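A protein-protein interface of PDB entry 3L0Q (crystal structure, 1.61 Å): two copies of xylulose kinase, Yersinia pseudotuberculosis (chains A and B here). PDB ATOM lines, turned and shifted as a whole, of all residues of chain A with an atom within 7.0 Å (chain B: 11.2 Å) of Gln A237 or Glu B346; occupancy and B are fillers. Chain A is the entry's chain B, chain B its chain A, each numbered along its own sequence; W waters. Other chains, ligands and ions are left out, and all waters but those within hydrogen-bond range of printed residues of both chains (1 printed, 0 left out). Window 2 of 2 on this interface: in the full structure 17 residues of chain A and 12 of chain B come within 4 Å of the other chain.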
ATOM      1  N   ALA A 175     -20.090 -22.076 -34.043  1.00  0.00           N
ATOM      2  CA  ALA A 175     -19.982 -20.625 -34.158  1.00  0.00           C
ATOM      3  C   ALA A 175     -20.738 -19.999 -35.348  1.00  0.00           C
ATOM      4  O   ALA A 175     -21.140 -18.827 -35.268  1.00  0.00           O
ATOM      5  CB  ALA A 175     -18.496 -20.228 -34.264  1.00  0.00           C
ATOM      6  N   LYS A 177     -22.956 -22.170 -37.862  1.00  0.00           N
ATOM      7  CA  LYS A 177     -23.876 -23.080 -38.562  1.00  0.00           C
ATOM      8  C   LYS A 177     -23.363 -23.687 -39.870  1.00  0.00           C
ATOM      9  O   LYS A 177     -24.074 -24.455 -40.517  1.00  0.00           O
ATOM     10  CB  LYS A 177     -25.238 -22.390 -38.859  1.00  0.00           C
ATOM     11  CG  LYS A 177     -25.810 -21.784 -37.590  1.00  0.00           C
ATOM     12  CD  LYS A 177     -27.231 -21.398 -37.836  1.00  0.00           C
ATOM     13  CE  LYS A 177     -27.688 -20.396 -36.823  1.00  0.00           C
ATOM     14  NZ  LYS A 177     -29.036 -19.981 -37.292  1.00  0.00           N
ATOM     15  N   GLY A 234     -20.366 -15.560 -41.156  1.00  0.00           N
ATOM     16  CA  GLY A 234     -19.722 -15.197 -39.921  1.00  0.00           C
ATOM     17  C   GLY A 234     -20.433 -15.691 -38.667  1.00  0.00           C
ATOM     18  O   GLY A 234     -21.190 -16.641 -38.712  1.00  0.00           O
ATOM     19  N   LEU A 235     -20.140 -15.046 -37.549  1.00  0.00           N
ATOM     20  CA  LEU A 235     -20.654 -15.482 -36.276  1.00  0.00           C
ATOM     21  C   LEU A 235     -22.168 -15.466 -36.330  1.00  0.00           C
ATOM     22  O   LEU A 235     -22.773 -14.443 -36.703  1.00  0.00           O
ATOM     23  CB  LEU A 235     -20.170 -14.526 -35.192  1.00  0.00           C
ATOM     24  CG  LEU A 235     -19.935 -15.125 -33.832  1.00  0.00           C
ATOM     25  CD1 LEU A 235     -19.078 -16.447 -33.894  1.00  0.00           C
ATOM     26  CD2 LEU A 235     -19.271 -14.032 -32.992  1.00  0.00           C
ATOM     27  N   SER A 236     -22.782 -16.591 -35.977  1.00  0.00           N
ATOM     28  CA  SER A 236     -24.235 -16.613 -35.963  1.00  0.00           C
ATOM     29  C   SER A 236     -24.819 -15.730 -34.874  1.00  0.00           C
ATOM     30  O   SER A 236     -24.169 -15.343 -33.902  1.00  0.00           O
ATOM     31  CB  SER A 236     -24.770 -18.025 -35.797  1.00  0.00           C
ATOM     32  OG  SER A 236     -24.463 -18.487 -34.492  1.00  0.00           O
ATOM     33  N   GLN A 237     -26.100 -15.446 -35.031  1.00  0.00           N
ATOM     34  CA  GLN A 237     -26.769 -14.679 -33.993  1.00  0.00           C
ATOM     35  C   GLN A 237     -26.663 -15.348 -32.657  1.00  0.00           C
ATOM     36  O   GLN A 237     -26.379 -14.702 -31.639  1.00  0.00           O
ATOM     37  CB  GLN A 237     -28.254 -14.489 -34.333  1.00  0.00           C
ATOM     38  CG  GLN A 237     -28.703 -13.113 -33.911  1.00  0.00           C
ATOM     39  CD  GLN A 237     -30.012 -12.695 -34.548  1.00  0.00           C
ATOM     40  OE1 GLN A 237     -30.711 -11.837 -34.010  1.00  0.00           O
ATOM     41  NE2 GLN A 237     -30.345 -13.285 -35.709  1.00  0.00           N
ATOM     42  N   ARG A 238     -26.894 -16.652 -32.647  1.00  0.00           N
ATOM     43  CA  ARG A 238     -26.842 -17.410 -31.425  1.00  0.00           C
ATOM     44  C   ARG A 238     -25.442 -17.367 -30.785  1.00  0.00           C
ATOM     45  O   ARG A 238     -25.299 -17.083 -29.609  1.00  0.00           O
ATOM     46  CB  ARG A 238     -27.221 -18.852 -31.673  1.00  0.00           C
ATOM     47  CG  ARG A 238     -27.341 -19.610 -30.408  1.00  0.00           C
ATOM     48  CD  ARG A 238     -27.280 -21.075 -30.703  1.00  0.00           C
ATOM     49  NE  ARG A 238     -27.662 -21.842 -29.531  1.00  0.00           N
ATOM     50  CZ  ARG A 238     -27.849 -23.154 -29.549  1.00  0.00           C
ATOM     51  NH1 ARG A 238     -27.650 -23.843 -30.682  1.00  0.00           N
ATOM     52  NH2 ARG A 238     -28.219 -23.769 -28.430  1.00  0.00           N
ATOM     53  N   ALA A 239     -24.422 -17.690 -31.574  1.00  0.00           N
ATOM     54  CA  ALA A 239     -23.058 -17.741 -31.058  1.00  0.00           C
ATOM     55  C   ALA A 239     -22.615 -16.344 -30.593  1.00  0.00           C
ATOM     56  O   ALA A 239     -21.921 -16.192 -29.573  1.00  0.00           O
ATOM     57  CB  ALA A 239     -22.131 -18.281 -32.171  1.00  0.00           C
ATOM     58  N   ALA A 240     -23.010 -15.311 -31.341  1.00  0.00           N
ATOM     59  CA  ALA A 240     -22.658 -13.953 -30.944  1.00  0.00           C
ATOM     60  C   ALA A 240     -23.233 -13.582 -29.585  1.00  0.00           C
ATOM     61  O   ALA A 240     -22.557 -12.950 -28.779  1.00  0.00           O
ATOM     62  CB  ALA A 240     -23.070 -12.913 -32.031  1.00  0.00           C
ATOM     63  N   SER A 241     -24.475 -13.995 -29.310  1.00  0.00           N
ATOM     64  CA  SER A 241     -25.065 -13.712 -28.014  1.00  0.00           C
ATOM     65  C   SER A 241     -24.368 -14.493 -26.909  1.00  0.00           C
ATOM     66  O   SER A 241     -24.150 -13.954 -25.803  1.00  0.00           O
ATOM     67  CB  SER A 241     -26.582 -13.992 -28.029  1.00  0.00           C
ATOM     68  OG  SER A 241     -26.857 -15.366 -28.179  1.00  0.00           O
ATOM     69  N   GLU A 242     -23.984 -15.742 -27.197  1.00  0.00           N
ATOM     70  CA  GLU A 242     -23.314 -16.584 -26.214  1.00  0.00           C
ATOM     71  C   GLU A 242     -21.907 -16.083 -25.838  1.00  0.00           C
ATOM     72  O   GLU A 242     -21.462 -16.263 -24.687  1.00  0.00           O
ATOM     73  CB  GLU A 242     -23.266 -18.027 -26.709  1.00  0.00           C
ATOM     74  CG  GLU A 242     -24.651 -18.668 -26.810  1.00  0.00           C
ATOM     75  CD  GLU A 242     -24.708 -19.952 -27.666  1.00  0.00           C
ATOM     76  OE1 GLU A 242     -23.830 -20.245 -28.499  1.00  0.00           O
ATOM     77  OE2 GLU A 242     -25.690 -20.691 -27.511  1.00  0.00           O
ATOM     78  N   LEU A 245     -20.234 -11.115 -28.576  1.00  0.00           N
ATOM     79  CA  LEU A 245     -19.634 -10.508 -29.770  1.00  0.00           C
ATOM     80  C   LEU A 245     -20.704 -10.086 -30.777  1.00  0.00           C
ATOM     81  O   LEU A 245     -21.914 -10.226 -30.520  1.00  0.00           O
ATOM     82  CB  LEU A 245     -18.643 -11.485 -30.419  1.00  0.00           C
ATOM     83  CG  LEU A 245     -17.419 -11.782 -29.524  1.00  0.00           C
ATOM     84  CD1 LEU A 245     -16.487 -12.730 -30.264  1.00  0.00           C
ATOM     85  CD2 LEU A 245     -16.671 -10.498 -29.208  1.00  0.00           C
ATOM     86  N   ILE A 246     -20.283  -9.593 -31.942  1.00  0.00           N
ATOM     87  CA  ILE A 246     -21.214  -9.047 -32.922  1.00  0.00           C
ATOM     88  C   ILE A 246     -21.550 -10.086 -33.970  1.00  0.00           C
ATOM     89  O   ILE A 246     -20.655 -10.692 -34.555  1.00  0.00           O
ATOM     90  CB  ILE A 246     -20.624  -7.807 -33.679  1.00  0.00           C
ATOM     91  CG1 ILE A 246     -20.171  -6.722 -32.715  1.00  0.00           C
ATOM     92  CG2 ILE A 246     -21.631  -7.278 -34.698  1.00  0.00           C
ATOM     93  CD1 ILE A 246     -21.266  -6.202 -31.832  1.00  0.00           C
ATOM     94  N   PRO A 247     -22.845 -10.306 -34.226  1.00  0.00           N
ATOM     95  CA  PRO A 247     -23.143 -11.279 -35.289  1.00  0.00           C
ATOM     96  C   PRO A 247     -22.492 -10.888 -36.611  1.00  0.00           C
ATOM     97  O   PRO A 247     -22.425  -9.697 -36.972  1.00  0.00           O
ATOM     98  CB  PRO A 247     -24.685 -11.217 -35.415  1.00  0.00           C
ATOM     99  CG  PRO A 247     -25.156 -10.672 -34.097  1.00  0.00           C
ATOM    100  CD  PRO A 247     -24.052  -9.784 -33.547  1.00  0.00           C
ATOM    101  N   GLY A 248     -22.014 -11.896 -37.345  1.00  0.00           N
ATOM    102  CA  GLY A 248     -21.435 -11.686 -38.662  1.00  0.00           C
ATOM    103  C   GLY A 248     -19.904 -11.515 -38.613  1.00  0.00           C
ATOM    104  O   GLY A 248     -19.230 -11.473 -39.675  1.00  0.00           O
ATOM    105  N   ILE B 335     -34.511  -7.304 -16.049  1.00  0.00           N
ATOM    106  CA  ILE B 335     -33.947  -7.035 -17.372  1.00  0.00           C
ATOM    107  C   ILE B 335     -34.004  -8.261 -18.286  1.00  0.00           C
ATOM    108  O   ILE B 335     -34.548  -8.202 -19.433  1.00  0.00           O
ATOM    109  CB  ILE B 335     -32.452  -6.530 -17.252  1.00  0.00           C
ATOM    110  CG1 ILE B 335     -32.432  -5.105 -16.732  1.00  0.00           C
ATOM    111  CG2 ILE B 335     -31.758  -6.461 -18.639  1.00  0.00           C
ATOM    112  CD1 ILE B 335     -31.050  -4.678 -16.286  1.00  0.00           C
ATOM    113  N   HIS B 338     -37.237  -9.912 -19.775  1.00  0.00           N
ATOM    114  CA  HIS B 338     -38.118  -9.155 -20.682  1.00  0.00           C
ATOM    115  C   HIS B 338     -37.916  -9.593 -22.139  1.00  0.00           C
ATOM    116  O   HIS B 338     -36.787  -9.768 -22.605  1.00  0.00           O
ATOM    117  CB  HIS B 338     -37.894  -7.638 -20.551  1.00  0.00           C
ATOM    118  CG  HIS B 338     -38.929  -6.820 -21.259  1.00  0.00           C
ATOM    119  ND1 HIS B 338     -39.987  -6.196 -20.608  1.00  0.00           N
ATOM    120  CD2 HIS B 338     -39.101  -6.562 -22.570  1.00  0.00           C
ATOM    121  CE1 HIS B 338     -40.733  -5.554 -21.495  1.00  0.00           C
ATOM    122  NE2 HIS B 338     -40.215  -5.770 -22.695  1.00  0.00           N
ATOM    123  N   PRO B 339     -39.002  -9.766 -22.875  1.00  0.00           N
ATOM    124  CA  PRO B 339     -38.834 -10.212 -24.269  1.00  0.00           C
ATOM    125  C   PRO B 339     -37.949  -9.319 -25.152  1.00  0.00           C
ATOM    126  O   PRO B 339     -37.411  -9.829 -26.158  1.00  0.00           O
ATOM    127  CB  PRO B 339     -40.261 -10.141 -24.843  1.00  0.00           C
ATOM    128  CG  PRO B 339     -41.140 -10.160 -23.651  1.00  0.00           C
ATOM    129  CD  PRO B 339     -40.428  -9.590 -22.501  1.00  0.00           C
ATOM    130  N   CYS B 340     -37.878  -8.028 -24.854  1.00  0.00           N
ATOM    131  CA  CYS B 340     -37.025  -7.131 -25.647  1.00  0.00           C
ATOM    132  C   CYS B 340     -35.528  -7.206 -25.315  1.00  0.00           C
ATOM    133  O   CYS B 340     -34.724  -6.518 -25.942  1.00  0.00           O
ATOM    134  CB  CYS B 340     -37.484  -5.699 -25.523  1.00  0.00           C
ATOM    135  SG  CYS B 340     -39.155  -5.464 -26.190  1.00  0.00           S
ATOM    136  N   TYR B 341     -35.161  -7.994 -24.317  1.00  0.00           N
ATOM    137  CA  TYR B 341     -33.779  -8.059 -23.881  1.00  0.00           C
ATOM    138  C   TYR B 341     -32.793  -8.486 -25.000  1.00  0.00           C
ATOM    139  O   TYR B 341     -31.792  -7.785 -25.240  1.00  0.00           O
ATOM    140  CB  TYR B 341     -33.643  -8.989 -22.685  1.00  0.00           C
ATOM    141  CG  TYR B 341     -32.208  -9.272 -22.271  1.00  0.00           C
ATOM    142  CD1 TYR B 341     -31.371  -8.251 -21.803  1.00  0.00           C
ATOM    143  CD2 TYR B 341     -31.694 -10.554 -22.339  1.00  0.00           C
ATOM    144  CE1 TYR B 341     -30.057  -8.515 -21.398  1.00  0.00           C
ATOM    145  CE2 TYR B 341     -30.376 -10.827 -21.932  1.00  0.00           C
ATOM    146  CZ  TYR B 341     -29.585  -9.807 -21.476  1.00  0.00           C
ATOM    147  OH  TYR B 341     -28.277 -10.064 -21.086  1.00  0.00           O
ATOM    148  N   PRO B 342     -33.080  -9.599 -25.683  1.00  0.00           N
ATOM    149  CA  PRO B 342     -32.028 -10.016 -26.645  1.00  0.00           C
ATOM    150  C   PRO B 342     -31.776  -8.995 -27.741  1.00  0.00           C
ATOM    151  O   PRO B 342     -30.595  -8.743 -28.113  1.00  0.00           O
ATOM    152  CB  PRO B 342     -32.568 -11.338 -27.227  1.00  0.00           C
ATOM    153  CG  PRO B 342     -33.467 -11.873 -26.169  1.00  0.00           C
ATOM    154  CD  PRO B 342     -34.113 -10.643 -25.524  1.00  0.00           C
ATOM    155  N   ALA B 343     -32.836  -8.422 -28.296  1.00  0.00           N
ATOM    156  CA  ALA B 343     -32.651  -7.387 -29.309  1.00  0.00           C
ATOM    157  C   ALA B 343     -31.882  -6.182 -28.754  1.00  0.00           C
ATOM    158  O   ALA B 343     -31.004  -5.624 -29.427  1.00  0.00           O
ATOM    159  CB  ALA B 343     -33.988  -6.960 -29.897  1.00  0.00           C
ATOM    160  N   LEU B 344     -32.223  -5.739 -27.535  1.00  0.00           N
ATOM    161  CA  LEU B 344     -31.565  -4.561 -26.990  1.00  0.00           C
ATOM    162  C   LEU B 344     -30.099  -4.839 -26.685  1.00  0.00           C
ATOM    163  O   LEU B 344     -29.270  -3.966 -26.908  1.00  0.00           O
ATOM    164  CB  LEU B 344     -32.282  -4.009 -25.725  1.00  0.00           C
ATOM    165  CG  LEU B 344     -31.770  -2.646 -25.285  1.00  0.00           C
ATOM    166  CD1 LEU B 344     -31.924  -1.603 -26.377  1.00  0.00           C
ATOM    167  CD2 LEU B 344     -32.567  -2.203 -23.974  1.00  0.00           C
ATOM    168  N   LEU B 345     -29.806  -6.038 -26.185  1.00  0.00           N
ATOM    169  CA  LEU B 345     -28.438  -6.454 -25.904  1.00  0.00           C
ATOM    170  C   LEU B 345     -27.590  -6.372 -27.201  1.00  0.00           C
ATOM    171  O   LEU B 345     -26.479  -5.825 -27.198  1.00  0.00           O
ATOM    172  CB  LEU B 345     -28.448  -7.864 -25.259  1.00  0.00           C
ATOM    173  CG  LEU B 345     -27.059  -8.398 -24.902  1.00  0.00           C
ATOM    174  CD1 LEU B 345     -26.389  -7.474 -23.891  1.00  0.00           C
ATOM    175  CD2 LEU B 345     -27.139  -9.861 -24.383  1.00  0.00           C
ATOM    176  N   GLU B 346     -28.165  -6.841 -28.298  1.00  0.00           N
ATOM    177  CA  GLU B 346     -27.470  -6.784 -29.614  1.00  0.00           C
ATOM    178  C   GLU B 346     -27.191  -5.341 -29.999  1.00  0.00           C
ATOM    179  O   GLU B 346     -26.083  -5.027 -30.447  1.00  0.00           O
ATOM    180  CB  GLU B 346     -28.272  -7.527 -30.700  1.00  0.00           C
ATOM    181  CG  GLU B 346     -27.485  -8.020 -31.934  1.00  0.00           C
ATOM    182  CD  GLU B 346     -28.402  -8.405 -33.084  1.00  0.00           C
ATOM    183  OE1 GLU B 346     -29.548  -8.824 -32.813  1.00  0.00           O
ATOM    184  OE2 GLU B 346     -28.007  -8.258 -34.268  1.00  0.00           O
ATOM    185  N   GLN B 347     -28.155  -4.436 -29.785  1.00  0.00           N
ATOM    186  CA  GLN B 347     -27.929  -3.037 -30.137  1.00  0.00           C
ATOM    187  C   GLN B 347     -26.916  -2.411 -29.165  1.00  0.00           C
ATOM    188  O   GLN B 347     -26.095  -1.565 -29.579  1.00  0.00           O
ATOM    189  CB  GLN B 347     -29.259  -2.241 -30.183  1.00  0.00           C
ATOM    190  CG  GLN B 347     -29.006  -0.722 -30.025  1.00  0.00           C
ATOM    191  CD  GLN B 347     -30.200   0.057 -29.463  1.00  0.00           C
ATOM    192  OE1 GLN B 347     -31.338  -0.073 -29.940  1.00  0.00           O
ATOM    193  NE2 GLN B 347     -29.938   0.865 -28.429  1.00  0.00           N
ATOM    194  N   ALA B 348     -26.972  -2.812 -27.882  1.00  0.00           N
ATOM    195  CA  ALA B 348     -25.998  -2.352 -26.914  1.00  0.00           C
ATOM    196  C   ALA B 348     -24.579  -2.696 -27.427  1.00  0.00           C
ATOM    197  O   ALA B 348     -23.722  -1.816 -27.527  1.00  0.00           O
ATOM    198  CB  ALA B 348     -26.247  -2.954 -25.522  1.00  0.00           C
ATOM    199  N   LYS B 349     -24.350  -3.955 -27.775  1.00  0.00           N
ATOM    200  CA  LYS B 349     -23.019  -4.366 -28.277  1.00  0.00           C
ATOM    201  C   LYS B 349     -22.595  -3.602 -29.530  1.00  0.00           C
ATOM    202  O   LYS B 349     -21.442  -3.163 -29.616  1.00  0.00           O
ATOM    203  CB  LYS B 349     -22.950  -5.867 -28.531  1.00  0.00           C
ATOM    204  CG  LYS B 349     -23.027  -6.660 -27.243  1.00  0.00           C
ATOM    205  CD  LYS B 349     -22.831  -8.137 -27.451  1.00  0.00           C
ATOM    206  CE  LYS B 349     -23.969  -8.703 -28.198  1.00  0.00           C
ATOM    207  NZ  LYS B 349     -23.848 -10.163 -28.383  1.00  0.00           N
ATOM    208  N   ASN B 350     -23.504  -3.412 -30.475  1.00  0.00           N
ATOM    209  CA  ASN B 350     -23.198  -2.564 -31.634  1.00  0.00           C
ATOM    210  C   ASN B 350     -22.738  -1.144 -31.300  1.00  0.00           C
ATOM    211  O   ASN B 350     -21.990  -0.555 -32.082  1.00  0.00           O
ATOM    212  CB  ASN B 350     -24.358  -2.521 -32.638  1.00  0.00           C
ATOM    213  CG  ASN B 350     -24.497  -3.817 -33.444  1.00  0.00           C
ATOM    214  OD1 ASN B 350     -23.545  -4.239 -34.092  1.00  0.00           O
ATOM    215  ND2 ASN B 350     -25.695  -4.395 -33.479  1.00  0.00           N
ATOM    216  N   LYS B 351     -23.185  -0.573 -30.175  1.00  0.00           N
ATOM    217  CA  LYS B 351     -22.735   0.758 -29.724  1.00  0.00           C
ATOM    218  C   LYS B 351     -21.614   0.727 -28.676  1.00  0.00           C
ATOM    219  O   LYS B 351     -21.226   1.767 -28.123  1.00  0.00           O
ATOM    220  CB  LYS B 351     -23.955   1.565 -29.201  1.00  0.00           C
ATOM    221  CG  LYS B 351     -24.945   1.891 -30.304  1.00  0.00           C
ATOM    222  CD  LYS B 351     -26.334   2.337 -29.806  1.00  0.00           C
ATOM    223  CE  LYS B 351     -26.307   3.660 -29.049  1.00  0.00           C
ATOM    224  NZ  LYS B 351     -27.729   4.222 -28.999  1.00  0.00           N
ATOM    225  N   GLY B 352     -21.133  -0.467 -28.351  1.00  0.00           N
ATOM    226  CA  GLY B 352     -20.087  -0.649 -27.358  1.00  0.00           C
ATOM    227  C   GLY B 352     -20.518  -0.287 -25.941  1.00  0.00           C
ATOM    228  O   GLY B 352     -19.775   0.343 -25.206  1.00  0.00           O
ATOM    229  N   GLU B 353     -21.716  -0.737 -25.570  1.00  0.00           N
ATOM    230  CA  GLU B 353     -22.443  -0.325 -24.375  1.00  0.00           C
ATOM    231  C   GLU B 353     -22.840  -1.578 -23.620  1.00  0.00           C
ATOM    232  O   GLU B 353     -23.028  -2.635 -24.233  1.00  0.00           O
ATOM    233  CB  GLU B 353     -23.775   0.344 -24.775  1.00  0.00           C
ATOM    234  CG  GLU B 353     -23.696   1.809 -24.968  1.00  0.00           C
ATOM    235  CD  GLU B 353     -25.024   2.430 -25.318  1.00  0.00           C
ATOM    236  OE1 GLU B 353     -26.059   1.714 -25.539  1.00  0.00           O
ATOM    237  OE2 GLU B 353     -25.019   3.672 -25.442  1.00  0.00           O
ATOM    238  N   THR B 354     -23.005  -1.433 -22.315  1.00  0.00           N
ATOM    239  CA  THR B 354     -23.673  -2.469 -21.501  1.00  0.00           C
ATOM    240  C   THR B 354     -25.193  -2.363 -21.647  1.00  0.00           C
ATOM    241  O   THR B 354     -25.695  -1.347 -22.089  1.00  0.00           O
ATOM    242  CB  THR B 354     -23.341  -2.323 -20.012  1.00  0.00           C
ATOM    243  OG1 THR B 354     -23.928  -1.107 -19.511  1.00  0.00           O
ATOM    244  CG2 THR B 354     -21.849  -2.288 -19.766  1.00  0.00           C
ATOM    245  N   ILE B 355     -25.925  -3.382 -21.183  1.00  0.00           N
ATOM    246  CA  ILE B 355     -27.378  -3.317 -21.282  1.00  0.00           C
ATOM    247  C   ILE B 355     -27.874  -2.181 -20.382  1.00  0.00           C
ATOM    248  O   ILE B 355     -28.855  -1.535 -20.721  1.00  0.00           O
ATOM    249  CB  ILE B 355     -28.042  -4.671 -20.898  1.00  0.00           C
ATOM    250  CG1 ILE B 355     -29.535  -4.661 -21.237  1.00  0.00           C
ATOM    251  CG2 ILE B 355     -27.813  -4.973 -19.450  1.00  0.00           C
ATOM    252  CD1 ILE B 355     -29.842  -4.823 -22.686  1.00  0.00           C
ATOM    253  N   TYR B 356     -27.216  -1.967 -19.241  1.00  0.00           N
ATOM    254  CA  TYR B 356     -27.582  -0.847 -18.339  1.00  0.00           C
ATOM    255  C   TYR B 356     -27.459   0.529 -19.021  1.00  0.00           C
ATOM    256  O   TYR B 356     -28.347   1.370 -18.886  1.00  0.00           O
ATOM    257  CB  TYR B 356     -26.796  -0.889 -17.022  1.00  0.00           C
ATOM    258  CG  TYR B 356     -26.700  -2.278 -16.502  1.00  0.00           C
ATOM    259  CD1 TYR B 356     -27.794  -2.871 -15.910  1.00  0.00           C
ATOM    260  CD2 TYR B 356     -25.532  -3.022 -16.633  1.00  0.00           C
ATOM    261  CE1 TYR B 356     -27.733  -4.164 -15.412  1.00  0.00           C
ATOM    262  CE2 TYR B 356     -25.468  -4.322 -16.191  1.00  0.00           C
ATOM    263  CZ  TYR B 356     -26.558  -4.882 -15.553  1.00  0.00           C
ATOM    264  OH  TYR B 356     -26.491  -6.179 -15.101  1.00  0.00           O
ATOM    265  N   ALA B 358     -27.625   1.047 -22.263  1.00  0.00           N
ATOM    266  CA  ALA B 358     -28.647   1.101 -23.299  1.00  0.00           C
ATOM    267  C   ALA B 358     -30.006   1.453 -22.675  1.00  0.00           C
ATOM    268  O   ALA B 358     -30.750   2.274 -23.225  1.00  0.00           O
ATOM    269  CB  ALA B 358     -28.731  -0.256 -24.063  1.00  0.00           C
ATOM    270  N   LEU B 359     -30.332   0.830 -21.532  1.00  0.00           N
ATOM    271  CA  LEU B 359     -31.591   1.211 -20.843  1.00  0.00           C
ATOM    272  C   LEU B 359     -31.556   2.654 -20.326  1.00  0.00           C
ATOM    273  O   LEU B 359     -32.571   3.410 -20.425  1.00  0.00           O
ATOM    274  CB  LEU B 359     -31.846   0.210 -19.730  1.00  0.00           C
ATOM    275  CG  LEU B 359     -32.127  -1.218 -20.178  1.00  0.00           C
ATOM    276  CD1 LEU B 359     -32.053  -2.180 -19.045  1.00  0.00           C
ATOM    277  CD2 LEU B 359     -33.567  -1.281 -20.753  1.00  0.00           C
ATOM    278  N   ILE B 362     -32.442   5.004 -23.071  1.00  0.00           N
ATOM    279  CA  ILE B 362     -33.862   5.015 -23.401  1.00  0.00           C
ATOM    280  C   ILE B 362     -34.553   5.885 -22.364  1.00  0.00           C
ATOM    281  O   ILE B 362     -35.398   6.705 -22.695  1.00  0.00           O
ATOM    282  CB  ILE B 362     -34.441   3.595 -23.401  1.00  0.00           C
ATOM    283  CG1 ILE B 362     -33.934   2.852 -24.671  1.00  0.00           C
ATOM    284  CG2 ILE B 362     -36.003   3.603 -23.377  1.00  0.00           C
ATOM    285  CD1 ILE B 362     -34.036   1.346 -24.558  1.00  0.00           C
ATOM    286  N   PRO B 411     -39.010  -1.748 -25.817  1.00  0.00           N
ATOM    287  CA  PRO B 411     -37.840  -1.430 -25.009  1.00  0.00           C
ATOM    288  C   PRO B 411     -38.173  -0.336 -23.987  1.00  0.00           C
ATOM    289  O   PRO B 411     -37.547  -0.346 -22.935  1.00  0.00           O
ATOM    290  CB  PRO B 411     -36.836  -0.885 -26.032  1.00  0.00           C
ATOM    291  CG  PRO B 411     -37.291  -1.395 -27.349  1.00  0.00           C
ATOM    292  CD  PRO B 411     -38.740  -1.673 -27.282  1.00  0.00           C
ATOM    293  N   MET B 414     -39.628  -2.037 -21.052  1.00  0.00           N
ATOM    294  CA  MET B 414     -38.552  -2.697 -20.355  1.00  0.00           C
ATOM    295  C   MET B 414     -37.770  -1.699 -19.483  1.00  0.00           C
ATOM    296  O   MET B 414     -37.424  -2.013 -18.330  1.00  0.00           O
ATOM    297  CB  MET B 414     -37.586  -3.355 -21.391  1.00  0.00           C
ATOM    298  CG  MET B 414     -36.456  -4.122 -20.721  1.00  0.00           C
ATOM    299  SD  MET B 414     -35.353  -4.882 -22.134  1.00  0.00           S
ATOM    300  CE  MET B 414     -33.850  -5.189 -21.100  1.00  0.00           C
HETATM  301  O   HOH W   1     -23.893 -11.201 -25.640  1.00  0.00           O
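O of Arg A238 lies within hydrogen-bond range of OG of Ser A241, 2.7 Å away.
O of Glu B346 sits at hydrogen-bond distance from ND2 of Asn B350.
The backbone NH of Leu A245 sits at hydrogen-bond distance from the backbone carbonyl oxygen of Ala A240 (3.0 Å).
Of the 15 printed residues of chain A, 6 touch a printed residue of chain B.
Hydrophobic or aromatic side chains of chain A that line the printed part of chain B: Ile A246 and Pro A247.
Among the printed residues, 7 pairs touch across the chains.
Among the printed residues, no Asp or Glu carboxylate lies within 4 Å of a Lys or Arg side-chain nitrogen of the other chain.
No position is printed for both chains.
Of chain B, only Glu B346 (3.4 Å) comes within 4 Å of Gln A237.
Glu B346 touches two residues of chain A.
No residue of chain B comes within 4 Å of Ser A236.
No residue of chain B comes within 4 Å of Ala A239.
Ala A240 touches just one residue of chain B: Lys B349.
Of chain B, only Glu B346 (3.7 Å) comes within 4 Å of Pro A247.
Of the printed residues of chain B, Ile A246 touches Lys B349 (3.7 Å) and Asn B350 (3.6 Å).
Of the printed residues of chain A, Asn B350 touches Ile A246 (3.6 Å).
Of the printed residues of chain A, Lys B349 touches Ala A240 (3.1 Å), Ser A241 (3.8 Å), Leu A245 (2.9 Å) and Ile A246 (3.7 Å).
Printed residues of chain B within 4 Å of Leu A245: Lys B349 (2.9 Å).
Printed residues of chain B within 4 Å of Ser A241: Lys B349 (3.8 Å).
The nearest residue of chain B that does not touch Gln A237 is Lys B349 (6.1 Å).
The side-chain carboxylate (OE1) of Glu B346 sits close to the side-chain amide oxygen (OE1) of Gln A237.
The side-chain amino group (NZ) of Lys B349 sits at hydrogen-bond distance from the backbone carbonyl oxygen (O) of Ala A240 (3.1 Å).
The backbone carbonyl oxygen of Leu A245 lies within hydrogen-bond range of the side-chain amino group of Lys B349, 2.9 Å away.
CA of Ser A241 touches NZ of Lys B349, 3.8 Å away.
CD1 of Ile A246 touches C of Lys B349 (3.7 Å).
Ile A246 touches Asn B350.
Pro A247 touches Glu B346.
Water W1 bridges O of Ser A241 (2.8 Å) and NZ of Lys B349 (2.9 Å).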
